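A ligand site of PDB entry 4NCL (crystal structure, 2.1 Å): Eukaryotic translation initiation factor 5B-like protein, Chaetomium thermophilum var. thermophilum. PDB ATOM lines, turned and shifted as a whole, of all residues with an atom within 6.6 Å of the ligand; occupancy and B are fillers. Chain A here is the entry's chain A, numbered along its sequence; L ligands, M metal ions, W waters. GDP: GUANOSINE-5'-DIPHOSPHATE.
The backbone carbonyl oxygen of His 18 lies close to an oxygen (O3B) of the ligand (3.3 Å). Merely in contact with the ligand: Val 19 and Arg 139. 15 residues have an atom within 4 Å of the ligand: His 18, Val 19, Asp 20, Thr 21, Gly 22, Lys 23, Thr 24, Lys 25, Asn 135, Lys 136, Asp 138, Arg 139, Ser 203, Ala 204 and His 205.
The side-chain hydroxyl (OG) of Ser 203 is in hydrogen-bond range of the side-chain carboxylate (OD2) of Asp 138, 2.5 Å away. The side-chain amide oxygen (OD1) of Asn 135 lies within hydrogen-bond range of the backbone NH (N) of Ala 204 (3.2 Å). NZ of Lys 23 sits at hydrogen-bond distance from O of His 18, at 2.7 Å. The side-chain amino group (NZ) of Lys 23 lies close to the backbone carbonyl oxygen (O) of Gly 17, at 3.5 Å. O of Asp 20 lies within hydrogen-bond range of NZ of Lys 136, 3.3 Å away. O of Val 105 lies within hydrogen-bond range of OG1 of Thr 21, at 3.1 Å. The side-chain amide oxygen (OD1) of Asn 135 is in hydrogen-bond range of the side-chain hydroxyl (OG1) of Thr 202 (2.8 Å). N of Thr 206 is in hydrogen-bond range of OG of Ser 203, 2.9 Å away.
The backbone NH (N) of Lys 25 lies within hydrogen-bond range of an oxygen (O1A) of the ligand (2.5 Å). The side-chain carboxylate (OD1) of Asp 138 lies within hydrogen-bond range of a nitrogen (N2) of the ligand, at 2.6 Å. The backbone NH (N) of Ala 204 lies within hydrogen-bond range of an oxygen (O6) of the ligand, at 2.7 Å. An oxygen (O3B) of the ligand lies close to the backbone NH of Lys 23, 3.4 Å away. O3B of the ligand lies within salt-bridge range of NZ of Lys 23 (2.7 Å). The backbone NH (N) of Asp 20 is in hydrogen-bond range of an oxygen (O1B) of the ligand. The backbone NH (N) of Thr 21 sits at hydrogen-bond distance from an oxygen (O3B) of the ligand, 2.8 Å away. N of Thr 24 is in hydrogen-bond range of O2B of the ligand. The side-chain hydroxyl of Thr 24 sits at hydrogen-bond distance from an oxygen (O2B) of the ligand. The backbone NH of Gly 22 sits at hydrogen-bond distance from an oxygen (O3B) of the ligand (2.9 Å). The backbone NH (N) of His 205 is in hydrogen-bond range of an oxygen (O6) of the ligand, 3.2 Å away. A nitrogen (N7) of the ligand lies within hydrogen-bond range of the side-chain amide nitrogen (ND2) of Asn 135 (3.3 Å). An oxygen (O6) of the ligand lies close to the backbone NH of Lys 136 (3.5 Å). The side-chain hydroxyl (OG) of Ser 203 lies close to an oxygen (O6) of the ligand, at 3.4 Å.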
ATOM      1  N   GLY A  17      -5.792 -16.741  19.406  1.00  0.00           N
ATOM      2  CA  GLY A  17      -6.746 -16.148  20.309  1.00  0.00           C
ATOM      3  C   GLY A  17      -7.019 -16.984  21.542  1.00  0.00           C
ATOM      4  O   GLY A  17      -6.832 -18.198  21.556  1.00  0.00           O
ATOM      5  N   HIS A  18      -7.462 -16.303  22.584  1.00  0.00           N
ATOM      6  CA  HIS A  18      -8.005 -16.942  23.775  1.00  0.00           C
ATOM      7  C   HIS A  18      -9.267 -17.699  23.368  1.00  0.00           C
ATOM      8  O   HIS A  18      -9.910 -17.346  22.385  1.00  0.00           O
ATOM      9  CB  HIS A  18      -8.298 -15.890  24.841  1.00  0.00           C
ATOM     10  CG  HIS A  18      -8.897 -16.437  26.092  1.00  0.00           C
ATOM     11  ND1 HIS A  18      -8.324 -17.459  26.817  1.00  0.00           N
ATOM     12  CD2 HIS A  18     -10.025 -16.081  26.768  1.00  0.00           C
ATOM     13  CE1 HIS A  18      -9.069 -17.725  27.874  1.00  0.00           C
ATOM     14  NE2 HIS A  18     -10.105 -16.906  27.871  1.00  0.00           N
ATOM     15  N   VAL A  19      -9.605 -18.764  24.088  1.00  0.00           N
ATOM     16  CA  VAL A  19     -10.819 -19.516  23.761  1.00  0.00           C
ATOM     17  C   VAL A  19     -12.021 -18.585  23.950  1.00  0.00           C
ATOM     18  O   VAL A  19     -11.981 -17.667  24.781  1.00  0.00           O
ATOM     19  CB  VAL A  19     -10.971 -20.798  24.618  1.00  0.00           C
ATOM     20  CG1 VAL A  19     -11.156 -20.452  26.087  1.00  0.00           C
ATOM     21  CG2 VAL A  19     -12.126 -21.650  24.121  1.00  0.00           C
ATOM     22  N   ASP A  20     -13.056 -18.765  23.121  1.00  0.00           N
ATOM     23  CA  ASP A  20     -14.308 -18.005  23.217  1.00  0.00           C
ATOM     24  C   ASP A  20     -14.130 -16.542  22.803  1.00  0.00           C
ATOM     25  O   ASP A  20     -14.983 -15.698  23.096  1.00  0.00           O
ATOM     26  CB  ASP A  20     -14.882 -18.100  24.635  1.00  0.00           C
ATOM     27  CG  ASP A  20     -16.400 -18.155  24.667  1.00  0.00           C
ATOM     28  OD1 ASP A  20     -17.041 -17.092  24.635  1.00  0.00           O
ATOM     29  OD2 ASP A  20     -16.939 -19.281  24.726  1.00  0.00           O
ATOM     30  N   THR A  21     -13.045 -16.246  22.093  1.00  0.00           N
ATOM     31  CA  THR A  21     -12.779 -14.890  21.628  1.00  0.00           C
ATOM     32  C   THR A  21     -13.379 -14.675  20.232  1.00  0.00           C
ATOM     33  O   THR A  21     -13.497 -13.533  19.766  1.00  0.00           O
ATOM     34  CB  THR A  21     -11.254 -14.592  21.591  1.00  0.00           C
ATOM     35  OG1 THR A  21     -11.024 -13.181  21.639  1.00  0.00           O
ATOM     36  CG2 THR A  21     -10.632 -15.187  20.340  1.00  0.00           C
ATOM     37  N   GLY A  22     -13.770 -15.767  19.597  1.00  0.00           N
ATOM     38  CA  GLY A  22     -14.409 -15.723  18.297  1.00  0.00           C
ATOM     39  C   GLY A  22     -13.480 -15.930  17.115  1.00  0.00           C
ATOM     40  O   GLY A  22     -13.805 -15.545  15.994  1.00  0.00           O
ATOM     41  N   LYS A  23     -12.324 -16.548  17.353  1.00  0.00           N
ATOM     42  CA  LYS A  23     -11.366 -16.811  16.283  1.00  0.00           C
ATOM     43  C   LYS A  23     -11.921 -17.806  15.262  1.00  0.00           C
ATOM     44  O   LYS A  23     -11.683 -17.661  14.062  1.00  0.00           O
ATOM     45  CB  LYS A  23     -10.021 -17.293  16.859  1.00  0.00           C
ATOM     46  CG  LYS A  23     -10.120 -18.287  17.996  1.00  0.00           C
ATOM     47  CD  LYS A  23      -8.760 -18.522  18.634  1.00  0.00           C
ATOM     48  CE  LYS A  23      -8.843 -19.656  19.641  1.00  0.00           C
ATOM     49  NZ  LYS A  23      -9.924 -19.446  20.644  1.00  0.00           N
ATOM     50  N   THR A  24     -12.600 -18.857  15.743  1.00  0.00           N
ATOM     51  CA  THR A  24     -13.168 -19.865  14.856  1.00  0.00           C
ATOM     52  C   THR A  24     -14.270 -19.241  14.001  1.00  0.00           C
ATOM     53  O   THR A  24     -14.287 -19.404  12.770  1.00  0.00           O
ATOM     54  CB  THR A  24     -13.761 -21.061  15.640  1.00  0.00           C
ATOM     55  OG1 THR A  24     -12.717 -21.765  16.326  1.00  0.00           O
ATOM     56  CG2 THR A  24     -14.478 -22.020  14.702  1.00  0.00           C
ATOM     57  N   LYS A  25     -15.163 -18.493  14.643  1.00  0.00           N
ATOM     58  CA  LYS A  25     -16.219 -17.807  13.909  1.00  0.00           C
ATOM     59  C   LYS A  25     -15.613 -16.800  12.953  1.00  0.00           C
ATOM     60  O   LYS A  25     -16.119 -16.605  11.848  1.00  0.00           O
ATOM     61  CB  LYS A  25     -17.195 -17.123  14.877  1.00  0.00           C
ATOM     62  CG  LYS A  25     -18.572 -16.841  14.294  1.00  0.00           C
ATOM     63  CD  LYS A  25     -19.373 -18.115  14.039  1.00  0.00           C
ATOM     64  CE  LYS A  25     -19.603 -18.888  15.322  1.00  0.00           C
ATOM     65  NZ  LYS A  25     -20.585 -19.984  15.135  1.00  0.00           N
ATOM     66  N   LEU A  26     -14.504 -16.190  13.356  1.00  0.00           N
ATOM     67  CA  LEU A  26     -13.862 -15.163  12.530  1.00  0.00           C
ATOM     68  C   LEU A  26     -13.292 -15.780  11.268  1.00  0.00           C
ATOM     69  O   LEU A  26     -13.544 -15.289  10.164  1.00  0.00           O
ATOM     70  CB  LEU A  26     -12.763 -14.440  13.312  1.00  0.00           C
ATOM     71  CG  LEU A  26     -12.100 -13.261  12.601  1.00  0.00           C
ATOM     72  CD1 LEU A  26     -13.156 -12.217  12.228  1.00  0.00           C
ATOM     73  CD2 LEU A  26     -11.037 -12.612  13.492  1.00  0.00           C
ATOM     74  N   ASP A  28     -14.157 -18.565   9.992  1.00  0.00           N
ATOM     75  CA  ASP A  28     -15.311 -19.039   9.239  1.00  0.00           C
ATOM     76  C   ASP A  28     -15.903 -17.918   8.394  1.00  0.00           C
ATOM     77  O   ASP A  28     -16.285 -18.141   7.241  1.00  0.00           O
ATOM     78  CB  ASP A  28     -16.365 -19.620  10.178  1.00  0.00           C
ATOM     79  CG  ASP A  28     -16.002 -21.022  10.675  1.00  0.00           C
ATOM     80  OD1 ASP A  28     -16.423 -21.378  11.802  1.00  0.00           O
ATOM     81  OD2 ASP A  28     -15.285 -21.751   9.960  1.00  0.00           O
ATOM     82  N   PRO A  83      -5.062 -22.328  17.263  1.00  0.00           N
ATOM     83  CA  PRO A  83      -5.618 -22.230  18.614  1.00  0.00           C
ATOM     84  C   PRO A  83      -4.667 -22.827  19.646  1.00  0.00           C
ATOM     85  O   PRO A  83      -4.311 -24.000  19.545  1.00  0.00           O
ATOM     86  CB  PRO A  83      -6.923 -23.014  18.521  1.00  0.00           C
ATOM     87  CG  PRO A  83      -6.629 -24.066  17.491  1.00  0.00           C
ATOM     88  CD  PRO A  83      -5.618 -23.488  16.532  1.00  0.00           C
ATOM     89  N   VAL A 105      -6.684 -12.346  18.180  1.00  0.00           N
ATOM     90  CA  VAL A 105      -8.095 -12.001  18.311  1.00  0.00           C
ATOM     91  C   VAL A 105      -8.409 -11.666  19.775  1.00  0.00           C
ATOM     92  O   VAL A 105      -8.122 -12.462  20.675  1.00  0.00           O
ATOM     93  CB  VAL A 105      -9.006 -13.148  17.834  1.00  0.00           C
ATOM     94  CG1 VAL A 105     -10.458 -12.708  17.870  1.00  0.00           C
ATOM     95  CG2 VAL A 105      -8.621 -13.582  16.410  1.00  0.00           C
ATOM     96  N   ASN A 135     -12.583  -7.967  18.138  1.00  0.00           N
ATOM     97  CA  ASN A 135     -13.751  -8.647  17.624  1.00  0.00           C
ATOM     98  C   ASN A 135     -15.035  -8.359  18.392  1.00  0.00           C
ATOM     99  O   ASN A 135     -14.996  -7.833  19.520  1.00  0.00           O
ATOM    100  CB  ASN A 135     -13.477 -10.150  17.615  1.00  0.00           C
ATOM    101  CG  ASN A 135     -14.391 -10.892  16.669  1.00  0.00           C
ATOM    102  OD1 ASN A 135     -14.733 -10.389  15.589  1.00  0.00           O
ATOM    103  ND2 ASN A 135     -14.804 -12.079  17.077  1.00  0.00           N
ATOM    104  N   LYS A 136     -16.159  -8.723  17.765  1.00  0.00           N
ATOM    105  CA  LYS A 136     -17.501  -8.621  18.330  1.00  0.00           C
ATOM    106  C   LYS A 136     -17.974  -7.193  18.532  1.00  0.00           C
ATOM    107  O   LYS A 136     -18.701  -6.908  19.493  1.00  0.00           O
ATOM    108  CB  LYS A 136     -17.598  -9.369  19.670  1.00  0.00           C
ATOM    109  CG  LYS A 136     -17.047 -10.800  19.666  1.00  0.00           C
ATOM    110  CD  LYS A 136     -17.715 -11.625  20.765  1.00  0.00           C
ATOM    111  CE  LYS A 136     -16.936 -12.895  21.079  1.00  0.00           C
ATOM    112  NZ  LYS A 136     -17.324 -13.474  22.399  1.00  0.00           N
ATOM    113  N   ILE A 137     -17.620  -6.291  17.628  1.00  0.00           N
ATOM    114  CA  ILE A 137     -18.082  -4.902  17.740  1.00  0.00           C
ATOM    115  C   ILE A 137     -19.601  -4.773  17.585  1.00  0.00           C
ATOM    116  O   ILE A 137     -20.183  -3.767  17.965  1.00  0.00           O
ATOM    117  CB  ILE A 137     -17.411  -3.982  16.703  1.00  0.00           C
ATOM    118  CG1 ILE A 137     -17.606  -4.540  15.291  1.00  0.00           C
ATOM    119  CG2 ILE A 137     -15.935  -3.798  17.027  1.00  0.00           C
ATOM    120  CD1 ILE A 137     -16.919  -3.716  14.230  1.00  0.00           C
ATOM    121  N   ASP A 138     -20.237  -5.799  17.025  1.00  0.00           N
ATOM    122  CA  ASP A 138     -21.691  -5.795  16.864  1.00  0.00           C
ATOM    123  C   ASP A 138     -22.387  -5.919  18.218  1.00  0.00           C
ATOM    124  O   ASP A 138     -23.586  -5.663  18.339  1.00  0.00           O
ATOM    125  CB  ASP A 138     -22.128  -6.931  15.944  1.00  0.00           C
ATOM    126  CG  ASP A 138     -21.695  -8.288  16.457  1.00  0.00           C
ATOM    127  OD1 ASP A 138     -22.540  -8.997  17.049  1.00  0.00           O
ATOM    128  OD2 ASP A 138     -20.510  -8.646  16.270  1.00  0.00           O
ATOM    129  N   ARG A 139     -21.622  -6.301  19.235  1.00  0.00           N
ATOM    130  CA  ARG A 139     -22.164  -6.397  20.586  1.00  0.00           C
ATOM    131  C   ARG A 139     -22.285  -5.017  21.227  1.00  0.00           C
ATOM    132  O   ARG A 139     -22.872  -4.883  22.305  1.00  0.00           O
ATOM    133  CB  ARG A 139     -21.284  -7.297  21.463  1.00  0.00           C
ATOM    134  CG  ARG A 139     -21.219  -8.755  21.027  1.00  0.00           C
ATOM    135  CD  ARG A 139     -21.946  -9.662  22.007  1.00  0.00           C
ATOM    136  NE  ARG A 139     -21.921  -9.128  23.371  1.00  0.00           N
ATOM    137  CZ  ARG A 139     -20.996  -9.404  24.280  1.00  0.00           C
ATOM    138  NH1 ARG A 139     -21.059  -8.851  25.483  1.00  0.00           N
ATOM    139  NH2 ARG A 139     -19.991 -10.222  23.998  1.00  0.00           N
ATOM    140  N   THR A 202     -13.575  -5.703  14.406  1.00  0.00           N
ATOM    141  CA  THR A 202     -14.166  -6.690  13.526  1.00  0.00           C
ATOM    142  C   THR A 202     -15.417  -7.258  14.151  1.00  0.00           C
ATOM    143  O   THR A 202     -15.643  -7.132  15.357  1.00  0.00           O
ATOM    144  CB  THR A 202     -13.204  -7.881  13.242  1.00  0.00           C
ATOM    145  OG1 THR A 202     -12.949  -8.613  14.454  1.00  0.00           O
ATOM    146  CG2 THR A 202     -11.878  -7.408  12.631  1.00  0.00           C
ATOM    147  N   SER A 203     -16.238  -7.871  13.298  1.00  0.00           N
ATOM    148  CA  SER A 203     -17.344  -8.708  13.737  1.00  0.00           C
ATOM    149  C   SER A 203     -17.365 -10.021  12.962  1.00  0.00           C
ATOM    150  O   SER A 203     -17.616 -10.014  11.748  1.00  0.00           O
ATOM    151  CB  SER A 203     -18.677  -7.993  13.558  1.00  0.00           C
ATOM    152  OG  SER A 203     -19.765  -8.829  13.914  1.00  0.00           O
ATOM    153  N   ALA A 204     -17.122 -11.136  13.636  1.00  0.00           N
ATOM    154  CA  ALA A 204     -17.271 -12.428  12.989  1.00  0.00           C
ATOM    155  C   ALA A 204     -18.747 -12.635  12.648  1.00  0.00           C
ATOM    156  O   ALA A 204     -19.084 -13.398  11.745  1.00  0.00           O
ATOM    157  CB  ALA A 204     -16.755 -13.552  13.881  1.00  0.00           C
ATOM    158  N   HIS A 205     -19.615 -11.945  13.381  1.00  0.00           N
ATOM    159  CA  HIS A 205     -21.052 -12.010  13.113  1.00  0.00           C
ATOM    160  C   HIS A 205     -21.447 -11.354  11.792  1.00  0.00           C
ATOM    161  O   HIS A 205     -22.107 -11.970  10.955  1.00  0.00           O
ATOM    162  CB  HIS A 205     -21.808 -11.343  14.261  1.00  0.00           C
ATOM    163  CG  HIS A 205     -23.302 -11.438  14.146  1.00  0.00           C
ATOM    164  ND1 HIS A 205     -23.962 -12.634  13.914  1.00  0.00           N
ATOM    165  CD2 HIS A 205     -24.268 -10.493  14.227  1.00  0.00           C
ATOM    166  CE1 HIS A 205     -25.263 -12.414  13.866  1.00  0.00           C
ATOM    167  NE2 HIS A 205     -25.477 -11.116  14.045  1.00  0.00           N
ATOM    168  N   THR A 206     -21.023 -10.107  11.588  1.00  0.00           N
ATOM    169  CA  THR A 206     -21.506  -9.312  10.452  1.00  0.00           C
ATOM    170  C   THR A 206     -20.496  -9.217   9.311  1.00  0.00           C
ATOM    171  O   THR A 206     -20.857  -8.797   8.211  1.00  0.00           O
ATOM    172  CB  THR A 206     -21.874  -7.882  10.870  1.00  0.00           C
ATOM    173  OG1 THR A 206     -20.668  -7.156  11.115  1.00  0.00           O
ATOM    174  CG2 THR A 206     -22.716  -7.896  12.139  1.00  0.00           C
HETATM  175  PB  GDP L   1     -13.265 -19.333  19.813  1.00  0.00           P
HETATM  176  O1B GDP L   1     -13.484 -20.332  20.926  1.00  0.00           O
HETATM  177  O2B GDP L   1     -12.671 -20.006  18.606  1.00  0.00           O
HETATM  178  O3B GDP L   1     -12.340 -18.248  20.292  1.00  0.00           O
HETATM  179  O3A GDP L   1     -14.671 -18.670  19.416  1.00  0.00           O
HETATM  180  PA  GDP L   1     -15.730 -19.447  18.496  1.00  0.00           P
HETATM  181  O1A GDP L   1     -15.688 -18.933  17.076  1.00  0.00           O
HETATM  182  O2A GDP L   1     -15.485 -20.934  18.535  1.00  0.00           O
HETATM  183  O5' GDP L   1     -17.124 -19.084  19.193  1.00  0.00           O
HETATM  184  C5' GDP L   1     -17.228 -17.951  20.058  1.00  0.00           C
HETATM  185  C4' GDP L   1     -18.698 -17.696  20.328  1.00  0.00           C
HETATM  186  O4' GDP L   1     -18.886 -16.280  20.317  1.00  0.00           O
HETATM  187  C3' GDP L   1     -19.559 -18.291  19.214  1.00  0.00           C
HETATM  188  O3' GDP L   1     -20.603 -19.092  19.774  1.00  0.00           O
HETATM  189  C2' GDP L   1     -20.144 -17.108  18.463  1.00  0.00           C
HETATM  190  O2' GDP L   1     -21.565 -17.253  18.397  1.00  0.00           O
HETATM  191  C1' GDP L   1     -19.775 -15.881  19.270  1.00  0.00           C
HETATM  192  N9  GDP L   1     -19.101 -14.869  18.417  1.00  0.00           N
HETATM  193  C8  GDP L   1     -17.889 -14.959  17.829  1.00  0.00           C
HETATM  194  N7  GDP L   1     -17.603 -13.834  17.129  1.00  0.00           N
HETATM  195  C5  GDP L   1     -18.645 -12.988  17.266  1.00  0.00           C
HETATM  196  C6  GDP L   1     -19.009 -11.624  16.807  1.00  0.00           C
HETATM  197  O6  GDP L   1     -18.252 -10.956  16.075  1.00  0.00           O
HETATM  198  N1  GDP L   1     -20.196 -11.130  17.190  1.00  0.00           N
HETATM  199  C2  GDP L   1     -21.049 -11.827  17.977  1.00  0.00           C
HETATM  200  N2  GDP L   1     -22.227 -11.266  18.318  1.00  0.00           N
HETATM  201  N3  GDP L   1     -20.771 -13.068  18.432  1.00  0.00           N
HETATM  202  C4  GDP L   1     -19.618 -13.682  18.123  1.00  0.00           C
HETATM  203 MG    MG M   1     -10.932 -22.089  18.322  1.00  0.00          MG
HETATM  204  O   HOH W   1     -17.567 -22.096  19.034  1.00  0.00           O
